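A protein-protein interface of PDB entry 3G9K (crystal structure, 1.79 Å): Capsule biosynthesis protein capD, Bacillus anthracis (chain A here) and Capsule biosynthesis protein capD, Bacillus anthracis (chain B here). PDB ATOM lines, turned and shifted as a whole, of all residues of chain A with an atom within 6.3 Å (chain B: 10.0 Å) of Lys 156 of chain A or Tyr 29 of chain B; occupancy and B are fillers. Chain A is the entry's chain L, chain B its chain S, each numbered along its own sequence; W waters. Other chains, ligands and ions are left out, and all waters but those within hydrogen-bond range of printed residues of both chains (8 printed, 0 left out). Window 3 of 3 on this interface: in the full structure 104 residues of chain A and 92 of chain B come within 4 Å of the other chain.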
ATOM      1  N   TYR A 153       9.437  -9.537  22.702  1.00  0.00           N
ATOM      2  CA  TYR A 153       9.100  -8.474  23.617  1.00  0.00           C
ATOM      3  C   TYR A 153       9.287  -7.127  22.927  1.00  0.00           C
ATOM      4  O   TYR A 153      10.365  -6.822  22.434  1.00  0.00           O
ATOM      5  CB  TYR A 153       9.936  -8.558  24.874  1.00  0.00           C
ATOM      6  CG  TYR A 153       9.636  -7.438  25.852  1.00  0.00           C
ATOM      7  CD1 TYR A 153       8.348  -7.180  26.249  1.00  0.00           C
ATOM      8  CD2 TYR A 153      10.639  -6.624  26.337  1.00  0.00           C
ATOM      9  CE1 TYR A 153       8.066  -6.156  27.136  1.00  0.00           C
ATOM     10  CE2 TYR A 153      10.372  -5.593  27.215  1.00  0.00           C
ATOM     11  CZ  TYR A 153       9.092  -5.362  27.618  1.00  0.00           C
ATOM     12  OH  TYR A 153       8.829  -4.327  28.514  1.00  0.00           O
ATOM     13  N   SER A 154       8.218  -6.353  22.883  1.00  0.00           N
ATOM     14  CA  SER A 154       8.154  -5.133  22.098  1.00  0.00           C
ATOM     15  C   SER A 154       7.353  -4.198  22.943  1.00  0.00           C
ATOM     16  O   SER A 154       6.881  -4.588  24.025  1.00  0.00           O
ATOM     17  CB  SER A 154       7.469  -5.379  20.724  1.00  0.00           C
ATOM     18  OG  SER A 154       6.073  -5.709  20.831  1.00  0.00           O
ATOM     19  N   ASP A 155       7.144  -2.980  22.458  1.00  0.00           N
ATOM     20  CA  ASP A 155       6.397  -2.006  23.248  1.00  0.00           C
ATOM     21  C   ASP A 155       4.890  -2.281  23.212  1.00  0.00           C
ATOM     22  O   ASP A 155       4.145  -1.639  23.932  1.00  0.00           O
ATOM     23  CB  ASP A 155       6.709  -0.553  22.814  1.00  0.00           C
ATOM     24  CG  ASP A 155       6.379  -0.266  21.354  1.00  0.00           C
ATOM     25  OD1 ASP A 155       5.890  -1.159  20.618  1.00  0.00           O
ATOM     26  OD2 ASP A 155       6.642   0.875  20.918  1.00  0.00           O
ATOM     27  N   LYS A 156       4.457  -3.223  22.372  1.00  0.00           N
ATOM     28  CA  LYS A 156       3.039  -3.569  22.240  1.00  0.00           C
ATOM     29  C   LYS A 156       2.559  -4.553  23.340  1.00  0.00           C
ATOM     30  O   LYS A 156       1.357  -4.768  23.481  1.00  0.00           O
ATOM     31  CB  LYS A 156       2.793  -4.254  20.890  1.00  0.00           C
ATOM     32  CG  LYS A 156       2.894  -3.401  19.599  1.00  0.00           C
ATOM     33  CD  LYS A 156       1.981  -4.052  18.532  1.00  0.00           C
ATOM     34  CE  LYS A 156       2.382  -3.740  17.102  1.00  0.00           C
ATOM     35  NZ  LYS A 156       1.528  -4.469  16.104  1.00  0.00           N
ATOM     36  N   LEU A 157       3.495  -5.131  24.097  1.00  0.00           N
ATOM     37  CA  LEU A 157       3.243  -6.331  24.902  1.00  0.00           C
ATOM     38  C   LEU A 157       3.254  -6.064  26.418  1.00  0.00           C
ATOM     39  O   LEU A 157       3.495  -6.963  27.235  1.00  0.00           O
ATOM     40  CB  LEU A 157       4.275  -7.406  24.494  1.00  0.00           C
ATOM     41  CG  LEU A 157       3.835  -8.430  23.461  1.00  0.00           C
ATOM     42  CD1 LEU A 157       2.857  -7.925  22.406  1.00  0.00           C
ATOM     43  CD2 LEU A 157       5.019  -9.180  22.855  1.00  0.00           C
ATOM     44  N   SER A 158       2.932  -4.844  26.813  1.00  0.00           N
ATOM     45  CA  SER A 158       3.090  -4.488  28.213  1.00  0.00           C
ATOM     46  C   SER A 158       2.223  -5.335  29.141  1.00  0.00           C
ATOM     47  O   SER A 158       2.664  -5.652  30.227  1.00  0.00           O
ATOM     48  CB  SER A 158       2.793  -3.004  28.433  1.00  0.00           C
ATOM     49  OG  SER A 158       1.525  -2.714  27.896  1.00  0.00           O
ATOM     50  N   ILE A 159       1.014  -5.735  28.733  1.00  0.00           N
ATOM     51  CA  ILE A 159       0.179  -6.589  29.635  1.00  0.00           C
ATOM     52  C   ILE A 159       0.762  -7.958  30.002  1.00  0.00           C
ATOM     53  O   ILE A 159       0.413  -8.519  31.061  1.00  0.00           O
ATOM     54  CB  ILE A 159      -1.261  -6.818  29.136  1.00  0.00           C
ATOM     55  CG1 ILE A 159      -1.307  -7.744  27.904  1.00  0.00           C
ATOM     56  CG2 ILE A 159      -1.938  -5.545  28.809  1.00  0.00           C
ATOM     57  CD1 ILE A 159      -2.728  -7.940  27.406  1.00  0.00           C
ATOM     58  N   PHE A 160       1.607  -8.504  29.124  1.00  0.00           N
ATOM     59  CA  PHE A 160       2.271  -9.784  29.343  1.00  0.00           C
ATOM     60  C   PHE A 160       3.600  -9.659  30.064  1.00  0.00           C
ATOM     61  O   PHE A 160       4.118 -10.657  30.568  1.00  0.00           O
ATOM     62  CB  PHE A 160       2.536 -10.465  28.004  1.00  0.00           C
ATOM     63  CG  PHE A 160       1.303 -10.646  27.180  1.00  0.00           C
ATOM     64  CD1 PHE A 160       0.344 -11.592  27.544  1.00  0.00           C
ATOM     65  CD2 PHE A 160       1.089  -9.875  26.050  1.00  0.00           C
ATOM     66  CE1 PHE A 160      -0.795 -11.765  26.777  1.00  0.00           C
ATOM     67  CE2 PHE A 160      -0.047 -10.040  25.279  1.00  0.00           C
ATOM     68  CZ  PHE A 160      -0.979 -11.022  25.625  1.00  0.00           C
ATOM     69  N   GLN A 175      -7.206  -9.058  29.263  1.00  0.00           N
ATOM     70  CA  GLN A 175      -6.936  -8.854  27.813  1.00  0.00           C
ATOM     71  C   GLN A 175      -8.076  -8.084  27.118  1.00  0.00           C
ATOM     72  O   GLN A 175      -8.874  -8.646  26.341  1.00  0.00           O
ATOM     73  CB  GLN A 175      -6.669 -10.214  27.102  1.00  0.00           C
ATOM     74  CG  GLN A 175      -5.381 -10.915  27.533  1.00  0.00           C
ATOM     75  CD  GLN A 175      -5.171 -12.254  26.884  1.00  0.00           C
ATOM     76  OE1 GLN A 175      -4.479 -12.375  25.872  1.00  0.00           O
ATOM     77  NE2 GLN A 175      -5.761 -13.276  27.476  1.00  0.00           N
ATOM     78  N   ASP A 177      -8.125  -5.584  24.700  1.00  0.00           N
ATOM     79  CA  ASP A 177      -8.100  -5.558  23.230  1.00  0.00           C
ATOM     80  C   ASP A 177      -8.682  -6.834  22.647  1.00  0.00           C
ATOM     81  O   ASP A 177      -9.492  -6.763  21.711  1.00  0.00           O
ATOM     82  CB  ASP A 177      -6.678  -5.376  22.662  1.00  0.00           C
ATOM     83  CG  ASP A 177      -6.055  -4.007  22.976  1.00  0.00           C
ATOM     84  OD1 ASP A 177      -6.734  -3.118  23.492  1.00  0.00           O
ATOM     85  OD2 ASP A 177      -4.866  -3.811  22.626  1.00  0.00           O
ATOM     86  N   LEU A 178      -8.267  -7.990  23.168  1.00  0.00           N
ATOM     87  CA  LEU A 178      -8.806  -9.268  22.712  1.00  0.00           C
ATOM     88  C   LEU A 178     -10.309  -9.410  22.972  1.00  0.00           C
ATOM     89  O   LEU A 178     -11.026  -9.978  22.141  1.00  0.00           O
ATOM     90  CB  LEU A 178      -8.030 -10.473  23.311  1.00  0.00           C
ATOM     91  CG  LEU A 178      -8.423 -11.905  22.921  1.00  0.00           C
ATOM     92  CD1 LEU A 178      -8.348 -12.120  21.395  1.00  0.00           C
ATOM     93  CD2 LEU A 178      -7.522 -12.942  23.680  1.00  0.00           C
ATOM     94  N   LYS A 204      -2.126  -4.575   8.165  1.00  0.00           N
ATOM     95  CA  LYS A 204      -1.031  -3.685   8.476  1.00  0.00           C
ATOM     96  C   LYS A 204       0.104  -4.413   9.196  1.00  0.00           C
ATOM     97  O   LYS A 204       1.267  -4.173   8.903  1.00  0.00           O
ATOM     98  CB  LYS A 204      -1.525  -2.525   9.333  1.00  0.00           C
ATOM     99  CG  LYS A 204      -0.435  -1.562   9.663  1.00  0.00           C
ATOM    100  CD  LYS A 204      -0.802  -0.625  10.793  1.00  0.00           C
ATOM    101  CE  LYS A 204       0.482  -0.166  11.538  1.00  0.00           C
ATOM    102  NZ  LYS A 204       1.172  -1.346  12.170  1.00  0.00           N
ATOM    103  N   THR A 205      -0.231  -5.351  10.085  1.00  0.00           N
ATOM    104  CA  THR A 205       0.761  -5.961  10.944  1.00  0.00           C
ATOM    105  C   THR A 205       1.450  -7.101  10.211  1.00  0.00           C
ATOM    106  O   THR A 205       2.675  -7.238  10.316  1.00  0.00           O
ATOM    107  CB  THR A 205       0.124  -6.457  12.250  1.00  0.00           C
ATOM    108  OG1 THR A 205      -0.356  -5.311  13.001  1.00  0.00           O
ATOM    109  CG2 THR A 205       1.133  -7.215  13.081  1.00  0.00           C
ATOM    110  N   LEU B  20      -0.437 -22.035  16.589  1.00  0.00           N
ATOM    111  CA  LEU B  20       0.191 -20.853  16.021  1.00  0.00           C
ATOM    112  C   LEU B  20       1.531 -21.198  15.349  1.00  0.00           C
ATOM    113  O   LEU B  20       2.165 -20.384  14.775  1.00  0.00           O
ATOM    114  CB  LEU B  20       0.459 -19.803  17.071  1.00  0.00           C
ATOM    115  CG  LEU B  20      -0.664 -19.228  17.888  1.00  0.00           C
ATOM    116  CD1 LEU B  20      -0.157 -18.270  18.884  1.00  0.00           C
ATOM    117  CD2 LEU B  20      -1.715 -18.646  17.044  1.00  0.00           C
ATOM    118  N   PHE B  24       3.566 -18.317  20.784  1.00  0.00           N
ATOM    119  CA  PHE B  24       3.157 -16.987  20.303  1.00  0.00           C
ATOM    120  C   PHE B  24       3.414 -16.731  18.815  1.00  0.00           C
ATOM    121  O   PHE B  24       3.698 -15.591  18.432  1.00  0.00           O
ATOM    122  CB  PHE B  24       3.920 -15.894  21.048  1.00  0.00           C
ATOM    123  CG  PHE B  24       4.007 -16.124  22.494  1.00  0.00           C
ATOM    124  CD1 PHE B  24       5.081 -16.832  23.037  1.00  0.00           C
ATOM    125  CD2 PHE B  24       3.017 -15.683  23.327  1.00  0.00           C
ATOM    126  CE1 PHE B  24       5.158 -17.049  24.385  1.00  0.00           C
ATOM    127  CE2 PHE B  24       3.096 -15.893  24.685  1.00  0.00           C
ATOM    128  CZ  PHE B  24       4.177 -16.586  25.209  1.00  0.00           C
ATOM    129  N   GLY B  25       3.298 -17.745  17.958  1.00  0.00           N
ATOM    130  CA  GLY B  25       3.555 -17.555  16.539  1.00  0.00           C
ATOM    131  C   GLY B  25       4.838 -16.807  16.203  1.00  0.00           C
ATOM    132  O   GLY B  25       5.909 -17.091  16.758  1.00  0.00           O
ATOM    133  N   THR B  26       4.727 -15.839  15.299  1.00  0.00           N
ATOM    134  CA  THR B  26       5.798 -14.879  15.033  1.00  0.00           C
ATOM    135  C   THR B  26       6.045 -13.940  16.176  1.00  0.00           C
ATOM    136  O   THR B  26       7.091 -13.283  16.222  1.00  0.00           O
ATOM    137  CB  THR B  26       5.437 -13.986  13.838  1.00  0.00           C
ATOM    138  OG1 THR B  26       4.285 -13.215  14.152  1.00  0.00           O
ATOM    139  CG2 THR B  26       5.150 -14.804  12.646  1.00  0.00           C
ATOM    140  N   GLY B  27       5.099 -13.852  17.104  1.00  0.00           N
ATOM    141  CA  GLY B  27       5.161 -12.887  18.192  1.00  0.00           C
ATOM    142  C   GLY B  27       4.596 -11.545  17.791  1.00  0.00           C
ATOM    143  O   GLY B  27       4.407 -10.666  18.620  1.00  0.00           O
ATOM    144  N   LYS B  28       4.325 -11.363  16.504  1.00  0.00           N
ATOM    145  CA  LYS B  28       3.642 -10.154  16.062  1.00  0.00           C
ATOM    146  C   LYS B  28       2.229 -10.185  16.655  1.00  0.00           C
ATOM    147  O   LYS B  28       1.650 -11.249  16.837  1.00  0.00           O
ATOM    148  CB  LYS B  28       3.612 -10.071  14.536  1.00  0.00           C
ATOM    149  CG  LYS B  28       5.009  -9.910  13.901  1.00  0.00           C
ATOM    150  CD  LYS B  28       5.007  -8.843  12.803  1.00  0.00           C
ATOM    151  CE  LYS B  28       6.404  -8.552  12.267  1.00  0.00           C
ATOM    152  NZ  LYS B  28       6.921  -7.250  12.800  1.00  0.00           N
ATOM    153  N   TYR B  29       1.713  -9.019  16.998  1.00  0.00           N
ATOM    154  CA  TYR B  29       0.537  -8.926  17.854  1.00  0.00           C
ATOM    155  C   TYR B  29      -0.314  -7.747  17.445  1.00  0.00           C
ATOM    156  O   TYR B  29       0.186  -6.627  17.307  1.00  0.00           O
ATOM    157  CB  TYR B  29       1.016  -8.738  19.275  1.00  0.00           C
ATOM    158  CG  TYR B  29      -0.015  -8.546  20.338  1.00  0.00           C
ATOM    159  CD1 TYR B  29      -0.558  -9.633  21.005  1.00  0.00           C
ATOM    160  CD2 TYR B  29      -0.359  -7.279  20.778  1.00  0.00           C
ATOM    161  CE1 TYR B  29      -1.457  -9.452  22.048  1.00  0.00           C
ATOM    162  CE2 TYR B  29      -1.258  -7.099  21.795  1.00  0.00           C
ATOM    163  CZ  TYR B  29      -1.809  -8.194  22.433  1.00  0.00           C
ATOM    164  OH  TYR B  29      -2.672  -8.010  23.491  1.00  0.00           O
ATOM    165  N   THR B  30      -1.583  -8.005  17.166  1.00  0.00           N
ATOM    166  CA  THR B  30      -2.491  -6.937  16.833  1.00  0.00           C
ATOM    167  C   THR B  30      -3.904  -7.315  17.269  1.00  0.00           C
ATOM    168  O   THR B  30      -4.230  -8.512  17.402  1.00  0.00           O
ATOM    169  CB  THR B  30      -2.411  -6.522  15.314  1.00  0.00           C
ATOM    170  OG1 THR B  30      -2.896  -5.169  15.154  1.00  0.00           O
ATOM    171  CG2 THR B  30      -3.187  -7.513  14.414  1.00  0.00           C
ATOM    172  N   ALA B  31      -4.723  -6.292  17.546  1.00  0.00           N
ATOM    173  CA  ALA B  31      -6.152  -6.524  17.873  1.00  0.00           C
ATOM    174  C   ALA B  31      -6.283  -7.548  19.013  1.00  0.00           C
ATOM    175  O   ALA B  31      -7.254  -8.278  19.085  1.00  0.00           O
ATOM    176  CB  ALA B  31      -6.912  -6.982  16.616  1.00  0.00           C
ATOM    177  N   GLY B  32      -5.284  -7.584  19.900  1.00  0.00           N
ATOM    178  CA  GLY B  32      -5.317  -8.411  21.089  1.00  0.00           C
ATOM    179  C   GLY B  32      -4.875  -9.828  20.921  1.00  0.00           C
ATOM    180  O   GLY B  32      -4.980 -10.620  21.846  1.00  0.00           O
ATOM    181  N   PHE B  33      -4.319 -10.158  19.770  1.00  0.00           N
ATOM    182  CA  PHE B  33      -3.889 -11.550  19.547  1.00  0.00           C
ATOM    183  C   PHE B  33      -2.570 -11.652  18.798  1.00  0.00           C
ATOM    184  O   PHE B  33      -2.194 -10.729  18.075  1.00  0.00           O
ATOM    185  CB  PHE B  33      -5.002 -12.353  18.850  1.00  0.00           C
ATOM    186  CG  PHE B  33      -5.346 -11.865  17.471  1.00  0.00           C
ATOM    187  CD1 PHE B  33      -4.731 -12.421  16.345  1.00  0.00           C
ATOM    188  CD2 PHE B  33      -6.310 -10.886  17.288  1.00  0.00           C
ATOM    189  CE1 PHE B  33      -5.064 -11.991  15.079  1.00  0.00           C
ATOM    190  CE2 PHE B  33      -6.623 -10.433  16.001  1.00  0.00           C
ATOM    191  CZ  PHE B  33      -5.974 -11.001  14.909  1.00  0.00           C
ATOM    192  N   PHE B  34      -1.924 -12.816  18.939  1.00  0.00           N
ATOM    193  CA  PHE B  34      -0.669 -13.149  18.314  1.00  0.00           C
ATOM    194  C   PHE B  34      -0.895 -13.796  16.950  1.00  0.00           C
ATOM    195  O   PHE B  34      -1.778 -14.632  16.792  1.00  0.00           O
ATOM    196  CB  PHE B  34       0.152 -14.074  19.248  1.00  0.00           C
ATOM    197  CG  PHE B  34       0.795 -13.347  20.413  1.00  0.00           C
ATOM    198  CD1 PHE B  34       1.871 -12.495  20.211  1.00  0.00           C
ATOM    199  CD2 PHE B  34       0.319 -13.489  21.690  1.00  0.00           C
ATOM    200  CE1 PHE B  34       2.436 -11.779  21.273  1.00  0.00           C
ATOM    201  CE2 PHE B  34       0.898 -12.805  22.762  1.00  0.00           C
ATOM    202  CZ  PHE B  34       1.975 -11.964  22.547  1.00  0.00           C
ATOM    203  N   LEU B  35      -0.103 -13.395  15.958  1.00  0.00           N
ATOM    204  CA  LEU B  35      -0.171 -13.955  14.603  1.00  0.00           C
ATOM    205  C   LEU B  35       0.758 -15.130  14.389  1.00  0.00           C
ATOM    206  O   LEU B  35       1.939 -15.063  14.724  1.00  0.00           O
ATOM    207  CB  LEU B  35       0.159 -12.838  13.587  1.00  0.00           C
ATOM    208  CG  LEU B  35      -0.964 -11.801  13.467  1.00  0.00           C
ATOM    209  CD1 LEU B  35      -0.460 -10.484  12.823  1.00  0.00           C
ATOM    210  CD2 LEU B  35      -2.108 -12.347  12.674  1.00  0.00           C
ATOM    211  N   ASN B  36       0.228 -16.209  13.805  1.00  0.00           N
ATOM    212  CA  ASN B  36       0.953 -17.405  13.502  1.00  0.00           C
ATOM    213  C   ASN B  36       2.207 -17.139  12.684  1.00  0.00           C
ATOM    214  O   ASN B  36       2.271 -16.169  11.921  1.00  0.00           O
ATOM    215  CB  ASN B  36       0.056 -18.344  12.667  1.00  0.00           C
ATOM    216  CG  ASN B  36      -0.208 -17.794  11.256  1.00  0.00           C
ATOM    217  OD1 ASN B  36       0.588 -18.019  10.341  1.00  0.00           O
ATOM    218  ND2 ASN B  36      -1.317 -17.090  11.081  1.00  0.00           N
HETATM  219  O   HOH W   1       3.546  -6.544  16.271  1.00  0.00           O
HETATM  220  O   HOH W   2      -2.387  -3.298  13.072  1.00  0.00           O
HETATM  221  O   HOH W   3      -3.896 -13.220  23.301  1.00  0.00           O
HETATM  222  O   HOH W   4      -0.888  -3.373  16.418  1.00  0.00           O
HETATM  223  O   HOH W   5      -4.232  -9.940  24.546  1.00  0.00           O
HETATM  224  O   HOH W   6      -3.924  -4.962  20.411  1.00  0.00           O
HETATM  225  O   HOH W   7      -5.865  -7.944  24.856  1.00  0.00           O
HETATM  226  O   HOH W   8       4.470  -5.416  11.697  1.00  0.00           O
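Leu 157 of chain A touches Tyr 29 of chain B.
CD2 of Leu 157 of chain A touches CE1 of Phe 34 of chain B (3.99 Å).
Tyr 29 of chain B touches Ile 159 of chain A (OH to CD1, 3.9 Å).
CE1 of Tyr 29 of chain B touches CE2 of Phe 160 of chain A, at 3.6 Å.
Phe 160 of chain A touches Phe 34 of chain B (CE2 to CE2, 3.9 Å).
Asp 177 of chain A touches Ala 31 of chain B (O to O, 3.8 Å).
Asp 177 of chain A touches Gly 32 of chain B.
Leu 178 of chain A touches Gly 32 of chain B (CB to O, 3.4 Å).
Thr 205 of chain A touches Lys 28 of chain B.
CG2 of Thr 205 of chain A touches CD1 of Leu 35 of chain B, at 3.6 Å.
The backbone carbonyl oxygen (O) of Lys 28 of chain B is in hydrogen-bond range of the backbone NH (N) of Leu 35 of chain B (2.9 Å).
OG of Ser 154 of chain A sits close to N of Lys 156 of chain A (3.3 Å).
The side-chain hydroxyl (OG1) of Thr 26 of chain B is in hydrogen-bond range of the backbone NH (N) of Lys 28 of chain B (3.0 Å).
The backbone carbonyl oxygen of Leu 35 of chain B sits at hydrogen-bond distance from the backbone NH of Thr 26 of chain B, 3.0 Å away.
Printed residues of chain B that touch a printed residue of chain A: Lys 28, Tyr 29, Thr 30, Ala 31, Gly 32, Phe 34 and Leu 35.
Of the 13 printed residues of chain A, 7 touch a printed residue of chain B.
Among the printed residues, 12 pairs touch across the chains.
Among the printed residues, no Asp or Glu carboxylate lies within 4 Å of a Lys or Arg side-chain nitrogen of the other chain.
Lys 156 of chain A touches just one residue of chain B: Tyr 29 (2.8 Å).
Tyr 29 of chain B touches four residues of chain A.
No residue of chain B comes within 4 Å of Ser 154 of chain A.
No residue of chain B comes within 4 Å of Asp 155 of chain A.
Printed residues of chain A within 4 Å of Gly 32 of chain B: Asp 177 (3.7 Å) and Leu 178 (3.4 Å).
Printed residues of chain A within 4 Å of Phe 34 of chain B: Leu 157 and Phe 160.
Of the printed residues of chain A, Leu 35 of chain B touches Thr 205 (3.6 Å).
The nearest residue of chain B that does not touch Lys 156 of chain A is Thr 30 of chain B (4.5 Å).
The nearest printed residue of chain A that does not touch Thr 30 of chain B is Lys 156 of chain A (4.5 Å).
Water W6 lies within hydrogen-bond range of OD2 of Asp 177 of chain A (2.7 Å), N of Gly 32 of chain B (3.0 Å) and N of Ala 31 of chain B (3.3 Å).
Water W4 lies within hydrogen-bond range of the side-chain amino group (NZ) of Lys 156 of chain A (2.7 Å) and the side-chain hydroxyl (OG1) of Thr 30 of chain B (3.0 Å).
Water W5 lies within hydrogen-bond range of the side-chain hydroxyl (OH) of Tyr 29 of chain B (2.7 Å), the side-chain amide oxygen (OE1) of Gln 175 of chain A (2.8 Å) and the backbone carbonyl oxygen (O) of Gly 32 of chain B (2.9 Å).
Water W2 bridges OG1 of Thr 30 of chain B (2.8 Å) and OG1 of Thr 205 of chain A (2.9 Å).
Water W1 bridges NZ of Lys 156 of chain A (2.9 Å) and N of Tyr 29 of chain B (3.2 Å).
Water W8 bridges O of Thr 205 of chain A (2.9 Å) and NZ of Lys 28 of chain B (3.3 Å).
NZ of Lys 156 of chain A is in hydrogen-bond range of O of Tyr 29 of chain B.
OG1 of Thr 30 of chain B sits close to OG1 of Thr 205 of chain A.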
